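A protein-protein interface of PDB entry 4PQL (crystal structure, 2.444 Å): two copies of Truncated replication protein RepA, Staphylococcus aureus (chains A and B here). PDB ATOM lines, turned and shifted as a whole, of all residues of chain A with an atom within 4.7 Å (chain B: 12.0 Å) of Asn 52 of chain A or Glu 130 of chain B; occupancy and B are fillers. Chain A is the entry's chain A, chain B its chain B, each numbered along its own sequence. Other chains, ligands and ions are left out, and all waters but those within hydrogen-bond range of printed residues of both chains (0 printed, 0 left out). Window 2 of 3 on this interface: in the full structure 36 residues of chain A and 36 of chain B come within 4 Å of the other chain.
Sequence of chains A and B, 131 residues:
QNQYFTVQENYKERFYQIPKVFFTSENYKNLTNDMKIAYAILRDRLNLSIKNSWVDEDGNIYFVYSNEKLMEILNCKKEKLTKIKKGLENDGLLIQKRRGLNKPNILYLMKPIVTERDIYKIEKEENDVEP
The side-chain amide oxygen (OD1) of Asn 52 of chain A sits at hydrogen-bond distance from the backbone NH (N) of Glu 130 of chain B (3.0 Å).
O of Ser 49 of chain A lies within hydrogen-bond range of N of Trp 54 of chain A. O of Glu 123 of chain B sits at hydrogen-bond distance from ND2 of Asn 127 of chain B.
Among the printed residues, pairs that only touch across the chains: Leu 48 of chain A with Glu 126 of chain B (3.3 Å), Leu 48 of chain A with Asp 128 of chain B (3.4 Å), Leu 48 of chain A with Glu 125 of chain B (3.5 Å), Asn 52 of chain A with Val 129 of chain B (3.6 Å), Trp 54 of chain A with Glu 130 of chain B (3.8 Å) and Lys 51 of chain A with Asn 127 of chain B (3.97 Å).
Of the printed residues of chain B, Asn 52 of chain A touches Val 129 and Glu 130. Of the printed residues of chain A, Glu 130 of chain B touches Asn 52 and Trp 54. Leu 48 of chain A touches just these residues of chain B: Glu 125 (3.5 Å), Glu 126 (3.3 Å) and Asp 128 (3.4 Å). No residue of chain B comes within 4 Å of Ser 49 of chain A. No residue of chain B comes within 4 Å of Ser 53 of chain A. Trp 54 of chain A touches just one residue of chain B: Glu 130. Printed residues of chain A within 4 Å of Asn 127 of chain B: Lys 51. Printed residues of chain A within 4 Å of Glu 125 of chain B: Leu 48 (3.5 Å). Of the printed residues of chain A, Asp 128 of chain B touches Leu 48 (3.4 Å). Of the printed residues of chain A, Glu 126 of chain B touches Leu 48 (3.3 Å). Of the printed residues of chain B, Lys 51 of chain A touches Asn 127 (3.97 Å). Glu 123 of chain B touches none of the printed residues of chain A.
Of the 9 printed residues of chain B, 6 touch a printed residue of chain A. Hydrophobic or aromatic side chains of chain B that line the printed part of chain A: Val 129. Hydrophobic or aromatic side chains of chain A within 4 Å of the printed part of chain B: Leu 48 and Trp 54. Among the printed residues, 7 pairs touch across the chains.
No position is printed for both chains.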
ATOM      1  N   LEU A  48     -23.851 -19.029  -8.870  1.00  0.00           N
ATOM      2  CA  LEU A  48     -23.852 -19.563  -7.480  1.00  0.00           C
ATOM      3  C   LEU A  48     -23.678 -21.102  -7.430  1.00  0.00           C
ATOM      4  O   LEU A  48     -22.994 -21.626  -6.546  1.00  0.00           O
ATOM      5  CB  LEU A  48     -25.102 -19.189  -6.698  1.00  0.00           C
ATOM      6  CG  LEU A  48     -25.290 -17.730  -6.341  1.00  0.00           C
ATOM      7  CD1 LEU A  48     -26.648 -17.565  -5.707  1.00  0.00           C
ATOM      8  CD2 LEU A  48     -24.184 -17.320  -5.376  1.00  0.00           C
ATOM      9  N   SER A  49     -24.270 -21.819  -8.377  1.00  0.00           N
ATOM     10  CA  SER A  49     -24.175 -23.280  -8.409  1.00  0.00           C
ATOM     11  C   SER A  49     -22.746 -23.754  -8.577  1.00  0.00           C
ATOM     12  O   SER A  49     -22.359 -24.774  -8.001  1.00  0.00           O
ATOM     13  CB  SER A  49     -25.005 -23.851  -9.538  1.00  0.00           C
ATOM     14  OG  SER A  49     -26.365 -23.622  -9.299  1.00  0.00           O
ATOM     15  N   ILE A  50     -21.963 -23.039  -9.376  1.00  0.00           N
ATOM     16  CA  ILE A  50     -20.555 -23.412  -9.503  1.00  0.00           C
ATOM     17  C   ILE A  50     -19.862 -23.251  -8.158  1.00  0.00           C
ATOM     18  O   ILE A  50     -19.045 -24.093  -7.772  1.00  0.00           O
ATOM     19  CB  ILE A  50     -19.797 -22.596 -10.553  1.00  0.00           C
ATOM     20  CG1 ILE A  50     -20.444 -22.780 -11.922  1.00  0.00           C
ATOM     21  CG2 ILE A  50     -18.343 -23.049 -10.625  1.00  0.00           C
ATOM     22  CD1 ILE A  50     -19.841 -21.917 -12.973  1.00  0.00           C
ATOM     23  N   LYS A  51     -20.197 -22.194  -7.423  1.00  0.00           N
ATOM     24  CA  LYS A  51     -19.586 -22.072  -6.085  1.00  0.00           C
ATOM     25  C   LYS A  51     -20.003 -23.199  -5.113  1.00  0.00           C
ATOM     26  O   LYS A  51     -19.220 -23.604  -4.252  1.00  0.00           O
ATOM     27  CB  LYS A  51     -19.879 -20.702  -5.464  1.00  0.00           C
ATOM     28  CG  LYS A  51     -18.947 -19.614  -5.977  1.00  0.00           C
ATOM     29  CD  LYS A  51     -19.479 -18.225  -5.684  1.00  0.00           C
ATOM     30  CE  LYS A  51     -18.546 -17.156  -6.223  1.00  0.00           C
ATOM     31  NZ  LYS A  51     -18.720 -15.854  -5.517  1.00  0.00           N
ATOM     32  N   ASN A  52     -21.217 -23.711  -5.258  1.00  0.00           N
ATOM     33  CA  ASN A  52     -21.729 -24.765  -4.382  1.00  0.00           C
ATOM     34  C   ASN A  52     -21.250 -26.166  -4.766  1.00  0.00           C
ATOM     35  O   ASN A  52     -21.655 -27.152  -4.152  1.00  0.00           O
ATOM     36  CB  ASN A  52     -23.258 -24.744  -4.381  1.00  0.00           C
ATOM     37  CG  ASN A  52     -23.818 -23.522  -3.702  1.00  0.00           C
ATOM     38  OD1 ASN A  52     -23.092 -22.799  -3.024  1.00  0.00           O
ATOM     39  ND2 ASN A  52     -25.102 -23.254  -3.916  1.00  0.00           N
ATOM     40  N   SER A  53     -20.410 -26.246  -5.795  1.00  0.00           N
ATOM     41  CA  SER A  53     -19.964 -27.525  -6.355  1.00  0.00           C
ATOM     42  C   SER A  53     -21.147 -28.366  -6.849  1.00  0.00           C
ATOM     43  O   SER A  53     -21.132 -29.597  -6.787  1.00  0.00           O
ATOM     44  CB  SER A  53     -19.143 -28.319  -5.331  1.00  0.00           C
ATOM     45  OG  SER A  53     -17.838 -27.785  -5.185  1.00  0.00           O
ATOM     46  N   TRP A  54     -22.181 -27.667  -7.308  1.00  0.00           N
ATOM     47  CA  TRP A  54     -23.361 -28.273  -7.918  1.00  0.00           C
ATOM     48  C   TRP A  54     -23.093 -28.529  -9.405  1.00  0.00           C
ATOM     49  O   TRP A  54     -23.777 -27.995 -10.286  1.00  0.00           O
ATOM     50  CB  TRP A  54     -24.597 -27.393  -7.727  1.00  0.00           C
ATOM     51  CG  TRP A  54     -25.087 -27.319  -6.308  1.00  0.00           C
ATOM     52  CD1 TRP A  54     -24.649 -28.056  -5.244  1.00  0.00           C
ATOM     53  CD2 TRP A  54     -26.093 -26.438  -5.797  1.00  0.00           C
ATOM     54  NE1 TRP A  54     -25.336 -27.703  -4.111  1.00  0.00           N
ATOM     55  CE2 TRP A  54     -26.224 -26.708  -4.420  1.00  0.00           C
ATOM     56  CE3 TRP A  54     -26.893 -25.442  -6.371  1.00  0.00           C
ATOM     57  CZ2 TRP A  54     -27.130 -26.031  -3.611  1.00  0.00           C
ATOM     58  CZ3 TRP A  54     -27.789 -24.768  -5.567  1.00  0.00           C
ATOM     59  CH2 TRP A  54     -27.901 -25.064  -4.201  1.00  0.00           C
ATOM     60  N   GLU B 123     -25.673  -7.768  -3.152  1.00  0.00           N
ATOM     61  CA  GLU B 123     -24.555  -8.515  -2.561  1.00  0.00           C
ATOM     62  C   GLU B 123     -25.045  -9.807  -1.918  1.00  0.00           C
ATOM     63  O   GLU B 123     -24.427 -10.860  -2.070  1.00  0.00           O
ATOM     64  CB  GLU B 123     -23.808  -7.680  -1.508  1.00  0.00           C
ATOM     65  CG  GLU B 123     -22.849  -6.647  -2.066  1.00  0.00           C
ATOM     66  CD  GLU B 123     -22.095  -5.879  -0.982  1.00  0.00           C
ATOM     67  OE1 GLU B 123     -22.720  -5.428   0.008  1.00  0.00           O
ATOM     68  OE2 GLU B 123     -20.859  -5.742  -1.113  1.00  0.00           O
ATOM     69  N   LYS B 124     -26.174  -9.708  -1.225  1.00  0.00           N
ATOM     70  CA  LYS B 124     -26.819 -10.828  -0.557  1.00  0.00           C
ATOM     71  C   LYS B 124     -27.230 -11.904  -1.560  1.00  0.00           C
ATOM     72  O   LYS B 124     -27.013 -13.089  -1.330  1.00  0.00           O
ATOM     73  CB  LYS B 124     -28.043 -10.324   0.214  1.00  0.00           C
ATOM     74  CG  LYS B 124     -28.903 -11.398   0.847  1.00  0.00           C
ATOM     75  CD  LYS B 124     -29.687 -10.845   2.029  1.00  0.00           C
ATOM     76  CE  LYS B 124     -30.865 -11.751   2.385  1.00  0.00           C
ATOM     77  NZ  LYS B 124     -30.451 -13.074   2.937  1.00  0.00           N
ATOM     78  N   GLU B 125     -27.811 -11.473  -2.674  1.00  0.00           N
ATOM     79  CA  GLU B 125     -28.232 -12.364  -3.744  1.00  0.00           C
ATOM     80  C   GLU B 125     -27.041 -13.013  -4.446  1.00  0.00           C
ATOM     81  O   GLU B 125     -27.036 -14.212  -4.697  1.00  0.00           O
ATOM     82  CB  GLU B 125     -29.080 -11.579  -4.754  1.00  0.00           C
ATOM     83  CG  GLU B 125     -29.735 -12.409  -5.843  1.00  0.00           C
ATOM     84  CD  GLU B 125     -29.114 -12.191  -7.217  1.00  0.00           C
ATOM     85  OE1 GLU B 125     -28.467 -11.142  -7.438  1.00  0.00           O
ATOM     86  OE2 GLU B 125     -29.282 -13.072  -8.082  1.00  0.00           O
ATOM     87  N   GLU B 126     -26.037 -12.208  -4.762  1.00  0.00           N
ATOM     88  CA  GLU B 126     -24.875 -12.648  -5.527  1.00  0.00           C
ATOM     89  C   GLU B 126     -23.935 -13.553  -4.741  1.00  0.00           C
ATOM     90  O   GLU B 126     -23.068 -14.205  -5.318  1.00  0.00           O
ATOM     91  CB  GLU B 126     -24.108 -11.432  -6.066  1.00  0.00           C
ATOM     92  CG  GLU B 126     -24.739 -10.836  -7.318  1.00  0.00           C
ATOM     93  CD  GLU B 126     -23.956  -9.673  -7.897  1.00  0.00           C
ATOM     94  OE1 GLU B 126     -24.354  -9.166  -8.967  1.00  0.00           O
ATOM     95  OE2 GLU B 126     -22.950  -9.266  -7.281  1.00  0.00           O
ATOM     96  N   ASN B 127     -24.072 -13.563  -3.423  1.00  0.00           N
ATOM     97  CA  ASN B 127     -23.231 -14.421  -2.604  1.00  0.00           C
ATOM     98  C   ASN B 127     -24.075 -15.369  -1.764  1.00  0.00           C
ATOM     99  O   ASN B 127     -23.697 -15.735  -0.653  1.00  0.00           O
ATOM    100  CB  ASN B 127     -22.311 -13.569  -1.731  1.00  0.00           C
ATOM    101  CG  ASN B 127     -21.391 -12.683  -2.564  1.00  0.00           C
ATOM    102  OD1 ASN B 127     -20.413 -13.155  -3.150  1.00  0.00           O
ATOM    103  ND2 ASN B 127     -21.733 -11.403  -2.658  1.00  0.00           N
ATOM    104  N   ASP B 128     -25.213 -15.784  -2.318  1.00  0.00           N
ATOM    105  CA  ASP B 128     -26.118 -16.699  -1.627  1.00  0.00           C
ATOM    106  C   ASP B 128     -25.627 -18.129  -1.830  1.00  0.00           C
ATOM    107  O   ASP B 128     -26.194 -18.899  -2.606  1.00  0.00           O
ATOM    108  CB  ASP B 128     -27.551 -16.527  -2.140  1.00  0.00           C
ATOM    109  CG  ASP B 128     -28.564 -17.308  -1.323  1.00  0.00           C
ATOM    110  OD1 ASP B 128     -28.255 -17.671  -0.168  1.00  0.00           O
ATOM    111  OD2 ASP B 128     -29.673 -17.552  -1.841  1.00  0.00           O
ATOM    112  N   VAL B 129     -24.575 -18.469  -1.093  1.00  0.00           N
ATOM    113  CA  VAL B 129     -23.869 -19.738  -1.231  1.00  0.00           C
ATOM    114  C   VAL B 129     -24.268 -20.758  -0.172  1.00  0.00           C
ATOM    115  O   VAL B 129     -25.174 -20.517   0.623  1.00  0.00           O
ATOM    116  CB  VAL B 129     -22.343 -19.534  -1.169  1.00  0.00           C
ATOM    117  CG1 VAL B 129     -21.898 -18.560  -2.244  1.00  0.00           C
ATOM    118  CG2 VAL B 129     -21.928 -19.041   0.210  1.00  0.00           C
ATOM    119  N   GLU B 130     -23.575 -21.893  -0.175  1.00  0.00           N
ATOM    120  CA  GLU B 130     -23.844 -22.991   0.744  1.00  0.00           C
ATOM    121  C   GLU B 130     -22.539 -23.578   1.300  1.00  0.00           C
ATOM    122  O   GLU B 130     -21.457 -23.203   0.849  1.00  0.00           O
ATOM    123  CB  GLU B 130     -24.653 -24.070   0.015  1.00  0.00           C
ATOM    124  CG  GLU B 130     -26.129 -23.751  -0.101  1.00  0.00           C
ATOM    125  CD  GLU B 130     -27.002 -24.921   0.288  1.00  0.00           C
ATOM    126  OE1 GLU B 130     -26.570 -26.078   0.100  1.00  0.00           O
ATOM    127  OE2 GLU B 130     -28.115 -24.683   0.804  1.00  0.00           O
ATOM    128  N   PRO B 131     -22.630 -24.481   2.299  1.00  0.00           N
ATOM    129  CA  PRO B 131     -21.401 -25.116   2.799  1.00  0.00           C
ATOM    130  C   PRO B 131     -20.646 -25.912   1.736  1.00  0.00           C
ATOM    131  O   PRO B 131     -21.270 -26.649   0.980  1.00  0.00           O
ATOM    132  CB  PRO B 131     -21.916 -26.045   3.907  1.00  0.00           C
ATOM    133  CG  PRO B 131     -23.169 -25.394   4.376  1.00  0.00           C
ATOM    134  CD  PRO B 131     -23.794 -24.823   3.140  1.00  0.00           C
